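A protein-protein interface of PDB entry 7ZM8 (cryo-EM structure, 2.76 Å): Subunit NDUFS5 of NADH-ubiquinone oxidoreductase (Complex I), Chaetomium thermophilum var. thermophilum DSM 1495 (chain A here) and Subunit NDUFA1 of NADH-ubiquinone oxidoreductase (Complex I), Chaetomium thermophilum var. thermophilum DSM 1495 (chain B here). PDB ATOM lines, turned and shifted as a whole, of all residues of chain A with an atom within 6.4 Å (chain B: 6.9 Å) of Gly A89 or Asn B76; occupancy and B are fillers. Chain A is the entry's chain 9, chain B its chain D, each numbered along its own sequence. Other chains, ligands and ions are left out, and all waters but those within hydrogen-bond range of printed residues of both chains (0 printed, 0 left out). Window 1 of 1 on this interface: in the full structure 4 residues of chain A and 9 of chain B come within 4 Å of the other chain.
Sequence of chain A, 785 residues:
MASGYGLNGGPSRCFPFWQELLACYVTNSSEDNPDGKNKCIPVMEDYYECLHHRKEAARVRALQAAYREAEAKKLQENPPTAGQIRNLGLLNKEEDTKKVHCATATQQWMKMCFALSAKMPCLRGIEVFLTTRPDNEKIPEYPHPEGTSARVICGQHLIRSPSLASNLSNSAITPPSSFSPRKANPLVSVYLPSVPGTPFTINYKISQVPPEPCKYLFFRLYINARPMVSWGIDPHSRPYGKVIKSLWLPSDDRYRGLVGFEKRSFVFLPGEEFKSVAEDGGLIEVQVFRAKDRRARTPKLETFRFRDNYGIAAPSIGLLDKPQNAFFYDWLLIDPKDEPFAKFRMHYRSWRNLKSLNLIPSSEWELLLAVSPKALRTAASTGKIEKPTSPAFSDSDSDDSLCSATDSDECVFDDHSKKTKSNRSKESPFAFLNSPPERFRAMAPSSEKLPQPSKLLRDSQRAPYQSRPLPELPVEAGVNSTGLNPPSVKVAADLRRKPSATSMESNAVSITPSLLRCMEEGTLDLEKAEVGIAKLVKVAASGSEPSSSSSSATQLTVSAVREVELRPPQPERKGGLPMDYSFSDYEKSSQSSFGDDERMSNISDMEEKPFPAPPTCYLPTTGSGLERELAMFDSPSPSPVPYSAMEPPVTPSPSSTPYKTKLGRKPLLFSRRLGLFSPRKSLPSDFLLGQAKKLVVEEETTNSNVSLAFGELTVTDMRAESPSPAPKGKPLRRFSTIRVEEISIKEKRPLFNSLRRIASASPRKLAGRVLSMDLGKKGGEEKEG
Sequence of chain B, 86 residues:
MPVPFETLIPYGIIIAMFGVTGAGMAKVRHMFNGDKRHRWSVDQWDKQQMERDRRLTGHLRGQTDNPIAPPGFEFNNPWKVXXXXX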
ATOM      1  N   ILE A  85      17.817  -0.769   5.964  1.00  0.00           N
ATOM      2  CA  ILE A  85      17.166   0.530   5.597  1.00  0.00           C
ATOM      3  C   ILE A  85      18.152   1.372   4.783  1.00  0.00           C
ATOM      4  O   ILE A  85      17.974   2.597   4.737  1.00  0.00           O
ATOM      5  CB  ILE A  85      16.644   1.299   6.832  1.00  0.00           C
ATOM      6  CG1 ILE A  85      16.270   0.369   7.985  1.00  0.00           C
ATOM      7  CG2 ILE A  85      15.472   2.193   6.456  1.00  0.00           C
ATOM      8  CD1 ILE A  85      15.966   1.093   9.272  1.00  0.00           C
ATOM      9  N   ASN A  87      19.274  -0.395   2.008  1.00  0.00           N
ATOM     10  CA  ASN A  87      18.938  -1.098   0.785  1.00  0.00           C
ATOM     11  C   ASN A  87      17.510  -0.831   0.344  1.00  0.00           C
ATOM     12  O   ASN A  87      17.099  -1.317  -0.713  1.00  0.00           O
ATOM     13  CB  ASN A  87      19.164  -2.597   0.973  1.00  0.00           C
ATOM     14  CG  ASN A  87      20.625  -2.946   1.085  1.00  0.00           C
ATOM     15  OD1 ASN A  87      21.458  -2.413   0.355  1.00  0.00           O
ATOM     16  ND2 ASN A  87      20.951  -3.838   2.009  1.00  0.00           N
ATOM     17  N   LEU A  88      16.749  -0.135   1.198  1.00  0.00           N
ATOM     18  CA  LEU A  88      15.369   0.261   0.811  1.00  0.00           C
ATOM     19  C   LEU A  88      15.313   0.951  -0.550  1.00  0.00           C
ATOM     20  O   LEU A  88      16.131   1.860  -0.777  1.00  0.00           O
ATOM     21  CB  LEU A  88      14.852   1.204   1.900  1.00  0.00           C
ATOM     22  CG  LEU A  88      13.573   1.970   1.579  1.00  0.00           C
ATOM     23  CD1 LEU A  88      12.400   1.017   1.434  1.00  0.00           C
ATOM     24  CD2 LEU A  88      13.285   3.004   2.653  1.00  0.00           C
ATOM     25  N   GLY A  89      14.405   0.528  -1.423  1.00  0.00           N
ATOM     26  CA  GLY A  89      14.182   1.169  -2.701  1.00  0.00           C
ATOM     27  C   GLY A  89      15.296   1.006  -3.699  1.00  0.00           C
ATOM     28  O   GLY A  89      15.393   1.798  -4.636  1.00  0.00           O
ATOM     29  N   LEU A  90      16.165   0.020  -3.466  1.00  0.00           N
ATOM     30  CA  LEU A  90      17.266  -0.276  -4.415  1.00  0.00           C
ATOM     31  C   LEU A  90      16.765  -1.311  -5.414  1.00  0.00           C
ATOM     32  O   LEU A  90      15.845  -2.069  -5.056  1.00  0.00           O
ATOM     33  CB  LEU A  90      18.502  -0.741  -3.643  1.00  0.00           C
ATOM     34  CG  LEU A  90      19.588   0.314  -3.423  1.00  0.00           C
ATOM     35  CD1 LEU A  90      19.027   1.574  -2.786  1.00  0.00           C
ATOM     36  CD2 LEU A  90      20.722  -0.246  -2.583  1.00  0.00           C
ATOM     37  N   LEU A  91      17.358  -1.361  -6.602  1.00  0.00           N
ATOM     38  CA  LEU A  91      16.842  -2.158  -7.710  1.00  0.00           C
ATOM     39  C   LEU A  91      17.074  -3.657  -7.559  1.00  0.00           C
ATOM     40  O   LEU A  91      16.497  -4.427  -8.332  1.00  0.00           O
ATOM     41  CB  LEU A  91      17.458  -1.681  -9.029  1.00  0.00           C
ATOM     42  CG  LEU A  91      18.925  -1.998  -9.332  1.00  0.00           C
ATOM     43  CD1 LEU A  91      19.207  -1.776 -10.807  1.00  0.00           C
ATOM     44  CD2 LEU A  91      19.876  -1.158  -8.487  1.00  0.00           C
ATOM     45  N   LYS A  93      17.356  -5.244  -4.164  1.00  0.00           N
ATOM     46  CA  LYS A  93      17.160  -5.661  -2.781  1.00  0.00           C
ATOM     47  C   LYS A  93      15.685  -5.616  -2.401  1.00  0.00           C
ATOM     48  O   LYS A  93      15.330  -5.097  -1.338  1.00  0.00           O
ATOM     49  CB  LYS A  93      17.979  -4.779  -1.837  1.00  0.00           C
ATOM     50  CG  LYS A  93      19.458  -4.709  -2.175  1.00  0.00           C
ATOM     51  CD  LYS A  93      20.090  -6.089  -2.184  1.00  0.00           C
ATOM     52  CE  LYS A  93      21.605  -6.000  -2.173  1.00  0.00           C
ATOM     53  NZ  LYS A  93      22.091  -4.762  -2.841  1.00  0.00           N
ATOM     54  N   ASP A  96      14.564  -6.634   1.140  1.00  0.00           N
ATOM     55  CA  ASP A  96      14.763  -5.696   2.239  1.00  0.00           C
ATOM     56  C   ASP A  96      13.750  -4.561   2.210  1.00  0.00           C
ATOM     57  O   ASP A  96      13.362  -4.060   3.270  1.00  0.00           O
ATOM     58  CB  ASP A  96      16.186  -5.142   2.208  1.00  0.00           C
ATOM     59  CG  ASP A  96      17.205  -6.129   2.740  1.00  0.00           C
ATOM     60  OD1 ASP A  96      16.822  -6.995   3.553  1.00  0.00           O
ATOM     61  OD2 ASP A  96      18.387  -6.039   2.348  1.00  0.00           O
ATOM     62  N   THR A  97      13.319  -4.133   1.021  1.00  0.00           N
ATOM     63  CA  THR A  97      12.308  -3.084   0.948  1.00  0.00           C
ATOM     64  C   THR A  97      11.005  -3.540   1.581  1.00  0.00           C
ATOM     65  O   THR A  97      10.338  -2.764   2.274  1.00  0.00           O
ATOM     66  CB  THR A  97      12.068  -2.663  -0.501  1.00  0.00           C
ATOM     67  OG1 THR A  97      11.251  -3.640  -1.153  1.00  0.00           O
ATOM     68  CG2 THR A  97      13.379  -2.544  -1.242  1.00  0.00           C
ATOM     69  N   HIS A 101       9.139  -1.855   4.731  1.00  0.00           N
ATOM     70  CA  HIS A 101       7.732  -1.404   4.577  1.00  0.00           C
ATOM     71  C   HIS A 101       6.771  -2.287   5.375  1.00  0.00           C
ATOM     72  O   HIS A 101       5.609  -1.866   5.545  1.00  0.00           O
ATOM     73  CB  HIS A 101       7.351  -1.415   3.100  1.00  0.00           C
ATOM     74  CG  HIS A 101       8.111  -0.403   2.322  1.00  0.00           C
ATOM     75  ND1 HIS A 101       8.544   0.770   2.898  1.00  0.00           N
ATOM     76  CD2 HIS A 101       8.518  -0.379   1.037  1.00  0.00           C
ATOM     77  CE1 HIS A 101       9.189   1.477   2.003  1.00  0.00           C
ATOM     78  NE2 HIS A 101       9.185   0.797   0.850  1.00  0.00           N
ATOM     79  N   GLU B  51      23.092  12.557  -4.285  1.00  0.00           N
ATOM     80  CA  GLU B  51      22.277  11.952  -3.205  1.00  0.00           C
ATOM     81  C   GLU B  51      21.144  11.143  -3.826  1.00  0.00           C
ATOM     82  O   GLU B  51      20.766  10.131  -3.242  1.00  0.00           O
ATOM     83  CB  GLU B  51      21.905  13.019  -2.185  1.00  0.00           C
ATOM     84  CG  GLU B  51      23.053  13.381  -1.269  1.00  0.00           C
ATOM     85  CD  GLU B  51      22.655  14.177  -0.043  1.00  0.00           C
ATOM     86  OE1 GLU B  51      21.449  14.229   0.252  1.00  0.00           O
ATOM     87  OE2 GLU B  51      23.554  14.739   0.612  1.00  0.00           O
ATOM     88  N   ARG B  54      22.423   7.832  -5.017  1.00  0.00           N
ATOM     89  CA  ARG B  54      22.430   6.837  -3.912  1.00  0.00           C
ATOM     90  C   ARG B  54      21.010   6.352  -3.630  1.00  0.00           C
ATOM     91  O   ARG B  54      20.865   5.213  -3.174  1.00  0.00           O
ATOM     92  CB  ARG B  54      23.071   7.460  -2.668  1.00  0.00           C
ATOM     93  CG  ARG B  54      23.382   6.471  -1.555  1.00  0.00           C
ATOM     94  CD  ARG B  54      24.383   7.002  -0.552  1.00  0.00           C
ATOM     95  NE  ARG B  54      23.940   8.265   0.015  1.00  0.00           N
ATOM     96  CZ  ARG B  54      24.607   8.956   0.929  1.00  0.00           C
ATOM     97  NH1 ARG B  54      24.116  10.097   1.378  1.00  0.00           N
ATOM     98  NH2 ARG B  54      25.758   8.506   1.390  1.00  0.00           N
ATOM     99  N   ARG B  55      20.006   7.175  -3.904  1.00  0.00           N
ATOM    100  CA  ARG B  55      18.594   6.762  -3.718  1.00  0.00           C
ATOM    101  C   ARG B  55      18.234   5.677  -4.738  1.00  0.00           C
ATOM    102  O   ARG B  55      17.561   4.714  -4.335  1.00  0.00           O
ATOM    103  CB  ARG B  55      17.664   7.971  -3.815  1.00  0.00           C
ATOM    104  CG  ARG B  55      17.642   8.864  -2.586  1.00  0.00           C
ATOM    105  CD  ARG B  55      16.646   9.970  -2.853  1.00  0.00           C
ATOM    106  NE  ARG B  55      15.297   9.439  -2.946  1.00  0.00           N
ATOM    107  CZ  ARG B  55      14.261  10.107  -3.433  1.00  0.00           C
ATOM    108  NH1 ARG B  55      14.426  11.329  -3.901  1.00  0.00           N
ATOM    109  NH2 ARG B  55      13.065   9.549  -3.469  1.00  0.00           N
ATOM    110  N   LEU B  56      18.673   5.804  -5.993  1.00  0.00           N
ATOM    111  CA  LEU B  56      18.315   4.847  -7.030  1.00  0.00           C
ATOM    112  C   LEU B  56      19.218   3.620  -7.018  1.00  0.00           C
ATOM    113  O   LEU B  56      18.750   2.506  -7.268  1.00  0.00           O
ATOM    114  CB  LEU B  56      18.358   5.528  -8.397  1.00  0.00           C
ATOM    115  CG  LEU B  56      17.240   6.537  -8.667  1.00  0.00           C
ATOM    116  CD1 LEU B  56      17.645   7.555  -9.711  1.00  0.00           C
ATOM    117  CD2 LEU B  56      15.977   5.825  -9.079  1.00  0.00           C
ATOM    118  N   THR B  57      20.507   3.791  -6.737  1.00  0.00           N
ATOM    119  CA  THR B  57      21.463   2.697  -6.850  1.00  0.00           C
ATOM    120  C   THR B  57      22.125   2.294  -5.544  1.00  0.00           C
ATOM    121  O   THR B  57      22.548   1.146  -5.421  1.00  0.00           O
ATOM    122  CB  THR B  57      22.570   3.048  -7.857  1.00  0.00           C
ATOM    123  OG1 THR B  57      23.498   3.951  -7.248  1.00  0.00           O
ATOM    124  CG2 THR B  57      21.990   3.676  -9.114  1.00  0.00           C
ATOM    125  N   ALA B  69      11.348   4.274 -11.652  1.00  0.00           N
ATOM    126  CA  ALA B  69      12.071   4.101 -10.407  1.00  0.00           C
ATOM    127  C   ALA B  69      11.621   2.818  -9.708  1.00  0.00           C
ATOM    128  O   ALA B  69      10.464   2.404  -9.833  1.00  0.00           O
ATOM    129  CB  ALA B  69      11.855   5.303  -9.493  1.00  0.00           C
ATOM    130  N   PRO B  70      12.518   2.167  -8.974  1.00  0.00           N
ATOM    131  CA  PRO B  70      12.169   0.917  -8.297  1.00  0.00           C
ATOM    132  C   PRO B  70      11.191   1.162  -7.165  1.00  0.00           C
ATOM    133  O   PRO B  70      11.095   2.285  -6.650  1.00  0.00           O
ATOM    134  CB  PRO B  70      13.519   0.419  -7.768  1.00  0.00           C
ATOM    135  CG  PRO B  70      14.340   1.644  -7.640  1.00  0.00           C
ATOM    136  CD  PRO B  70      13.926   2.535  -8.762  1.00  0.00           C
ATOM    137  N   PRO B  71      10.434   0.142  -6.759  1.00  0.00           N
ATOM    138  CA  PRO B  71       9.515   0.318  -5.627  1.00  0.00           C
ATOM    139  C   PRO B  71      10.278   0.620  -4.348  1.00  0.00           C
ATOM    140  O   PRO B  71      11.373   0.105  -4.119  1.00  0.00           O
ATOM    141  CB  PRO B  71       8.772  -1.021  -5.545  1.00  0.00           C
ATOM    142  CG  PRO B  71       9.242  -1.842  -6.699  1.00  0.00           C
ATOM    143  CD  PRO B  71      10.501  -1.253  -7.216  1.00  0.00           C
ATOM    144  N   GLY B  72       9.682   1.462  -3.509  1.00  0.00           N
ATOM    145  CA  GLY B  72      10.339   1.964  -2.326  1.00  0.00           C
ATOM    146  C   GLY B  72      11.167   3.210  -2.544  1.00  0.00           C
ATOM    147  O   GLY B  72      11.651   3.789  -1.566  1.00  0.00           O
ATOM    148  N   PHE B  73      11.348   3.638  -3.794  1.00  0.00           N
ATOM    149  CA  PHE B  73      12.102   4.855  -4.064  1.00  0.00           C
ATOM    150  C   PHE B  73      11.392   6.089  -3.522  1.00  0.00           C
ATOM    151  O   PHE B  73      12.047   7.076  -3.168  1.00  0.00           O
ATOM    152  CB  PHE B  73      12.349   4.994  -5.567  1.00  0.00           C
ATOM    153  CG  PHE B  73      13.029   6.272  -5.948  1.00  0.00           C
ATOM    154  CD1 PHE B  73      14.383   6.444  -5.725  1.00  0.00           C
ATOM    155  CD2 PHE B  73      12.313   7.307  -6.515  1.00  0.00           C
ATOM    156  CE1 PHE B  73      15.006   7.620  -6.059  1.00  0.00           C
ATOM    157  CE2 PHE B  73      12.934   8.483  -6.856  1.00  0.00           C
ATOM    158  CZ  PHE B  73      14.282   8.642  -6.626  1.00  0.00           C
ATOM    159  N   GLU B  74      10.065   6.060  -3.442  1.00  0.00           N
ATOM    160  CA  GLU B  74       9.325   7.194  -2.912  1.00  0.00           C
ATOM    161  C   GLU B  74       9.421   7.317  -1.397  1.00  0.00           C
ATOM    162  O   GLU B  74       8.776   8.199  -0.825  1.00  0.00           O
ATOM    163  CB  GLU B  74       7.859   7.103  -3.331  1.00  0.00           C
ATOM    164  CG  GLU B  74       7.063   6.036  -2.604  1.00  0.00           C
ATOM    165  CD  GLU B  74       7.121   4.700  -3.300  1.00  0.00           C
ATOM    166  OE1 GLU B  74       8.018   4.507  -4.146  1.00  0.00           O
ATOM    167  OE2 GLU B  74       6.262   3.844  -3.010  1.00  0.00           O
ATOM    168  N   PHE B  75      10.212   6.469  -0.735  1.00  0.00           N
ATOM    169  CA  PHE B  75      10.368   6.505   0.711  1.00  0.00           C
ATOM    170  C   PHE B  75      11.789   6.760   1.189  1.00  0.00           C
ATOM    171  O   PHE B  75      11.960   7.198   2.329  1.00  0.00           O
ATOM    172  CB  PHE B  75       9.894   5.184   1.337  1.00  0.00           C
ATOM    173  CG  PHE B  75       8.459   4.859   1.058  1.00  0.00           C
ATOM    174  CD1 PHE B  75       7.446   5.599   1.628  1.00  0.00           C
ATOM    175  CD2 PHE B  75       8.127   3.809   0.230  1.00  0.00           C
ATOM    176  CE1 PHE B  75       6.133   5.300   1.373  1.00  0.00           C
ATOM    177  CE2 PHE B  75       6.817   3.507  -0.023  1.00  0.00           C
ATOM    178  CZ  PHE B  75       5.819   4.255   0.547  1.00  0.00           C
ATOM    179  N   ASN B  76      12.786   6.488   0.339  1.00  0.00           N
ATOM    180  CA  ASN B  76      14.218   6.581   0.736  1.00  0.00           C
ATOM    181  C   ASN B  76      14.786   7.997   0.578  1.00  0.00           C
ATOM    182  O   ASN B  76      16.015   8.132   0.651  1.00  0.00           O
ATOM    183  CB  ASN B  76      15.073   5.561  -0.020  1.00  0.00           C
ATOM    184  CG  ASN B  76      15.001   5.673  -1.528  1.00  0.00           C
ATOM    185  OD1 ASN B  76      14.586   6.692  -2.067  1.00  0.00           O
ATOM    186  ND2 ASN B  76      15.421   4.629  -2.220  1.00  0.00           N
ATOM    187  N   ASN B  77      13.935   9.005   0.392  1.00  0.00           N
ATOM    188  CA  ASN B  77      14.416  10.371   0.258  1.00  0.00           C
ATOM    189  C   ASN B  77      14.982  10.837   1.591  1.00  0.00           C
ATOM    190  O   ASN B  77      14.246  10.879   2.584  1.00  0.00           O
ATOM    191  CB  ASN B  77      13.278  11.275  -0.194  1.00  0.00           C
ATOM    192  CG  ASN B  77      13.762  12.609  -0.704  1.00  0.00           C
ATOM    193  OD1 ASN B  77      14.904  12.750  -1.128  1.00  0.00           O
ATOM    194  ND2 ASN B  77      12.887  13.604  -0.667  1.00  0.00           N
ATOM    195  N   PRO B  78      16.294  11.154   1.704  1.00  0.00           N
ATOM    196  CA  PRO B  78      16.876  11.428   3.006  1.00  0.00           C
ATOM    197  C   PRO B  78      16.564  12.825   3.525  1.00  0.00           C
ATOM    198  O   PRO B  78      16.808  13.780   2.830  1.00  0.00           O
ATOM    199  CB  PRO B  78      18.387  11.257   2.802  1.00  0.00           C
ATOM    200  CG  PRO B  78      18.566  10.848   1.358  1.00  0.00           C
ATOM    201  CD  PRO B  78      17.317  11.319   0.654  1.00  0.00           C
ATOM    202  N   TRP B  79      16.026  12.921   4.739  1.00  0.00           N
ATOM    203  CA  TRP B  79      15.935  14.266   5.357  1.00  0.00           C
ATOM    204  C   TRP B  79      16.975  14.345   6.467  1.00  0.00           C
ATOM    205  O   TRP B  79      16.780  13.689   7.495  1.00  0.00           O
ATOM    206  CB  TRP B  79      14.514  14.548   5.857  1.00  0.00           C
ATOM    207  CG  TRP B  79      13.514  14.888   4.794  1.00  0.00           C
ATOM    208  CD1 TRP B  79      13.622  14.660   3.454  1.00  0.00           C
ATOM    209  CD2 TRP B  79      12.233  15.516   4.989  1.00  0.00           C
ATOM    210  NE1 TRP B  79      12.505  15.104   2.803  1.00  0.00           N
ATOM    211  CE2 TRP B  79      11.635  15.635   3.718  1.00  0.00           C
ATOM    212  CE3 TRP B  79      11.534  15.983   6.107  1.00  0.00           C
ATOM    213  CZ2 TRP B  79      10.378  16.207   3.537  1.00  0.00           C
ATOM    214  CZ3 TRP B  79      10.292  16.546   5.928  1.00  0.00           C
ATOM    215  CH2 TRP B  79       9.724  16.658   4.659  1.00  0.00           C
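O of Phe B73 sits close to OD1 of Asn B76.
The backbone carbonyl oxygen (O) of Phe B73 is in hydrogen-bond range of the guanidinium group (NH2) of Arg B55, at 2.7 Å.
OD1 of Asn B76 sits at hydrogen-bond distance from NE of Arg B55 (3.0 Å).
The guanidinium group of Arg B55 is in hydrogen-bond range of the side-chain amide oxygen of Asn B77 (3.2 Å).
Along chain A the printed residues that touch a printed residue of chain B span positions 88 to 101.
Hydrophobic or aromatic side chains of chain B that line the printed part of chain A: Pro B70 and Phe B75.
Among the printed residues, 11 pairs touch across the chains.
O of Gly A89 touches O of Arg B55, at 3.6 Å.
CG of Pro B70 touches O of Gly A89, at 3.2 Å.
O of Pro B71 touches CA of Gly A89 (3.3 Å).
Gly B72 touches Gly A89 (C to CA, 3.6 Å).
Gly A89 touches Phe B73 (CA to N, 3.9 Å).
Asn B76 touches Gly A89.
Leu A90 touches Arg B55 (CD1 to O, 3.8 Å).
O of Thr B57 touches CD2 of Leu A90 (3.7 Å).
His A101 touches Gly B72 (NE2 to CA, 3.6 Å).
His A101 touches Phe B75 (CE1 to CD2, 3.1 Å).
Of the printed residues of chain B, Gly A89 touches Arg B55 (3.6 Å), Pro B70 (3.2 Å), Pro B71 (3.3 Å), Gly B72 (3.6 Å), Phe B73 (3.9 Å) and Asn B76 (3.7 Å).
Printed residues of chain B within 4 Å of Leu A90: Arg B55 (3.8 Å) and Thr B57 (3.7 Å).
Of the printed residues of chain B, His A101 touches Gly B72 (3.6 Å) and Phe B75 (3.1 Å).
Of the printed residues of chain A, Pro B71 touches Gly A89 (3.3 Å).
Of the printed residues of chain A, Gly B72 touches Gly A89 and His A101.
Printed residues of chain A within 4 Å of Phe B73: Gly A89.
Of chain A, only Leu A88 (3.2 Å) and Gly A89 (3.7 Å) come within 4 Å of Asn B76.
The nearest residue of chain A that does not touch Asn B76 is Leu A90 (4.8 Å).
The backbone carbonyl oxygen of Leu A88 sits at hydrogen-bond distance from the side-chain amide nitrogen of Asn B76 (3.2 Å).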
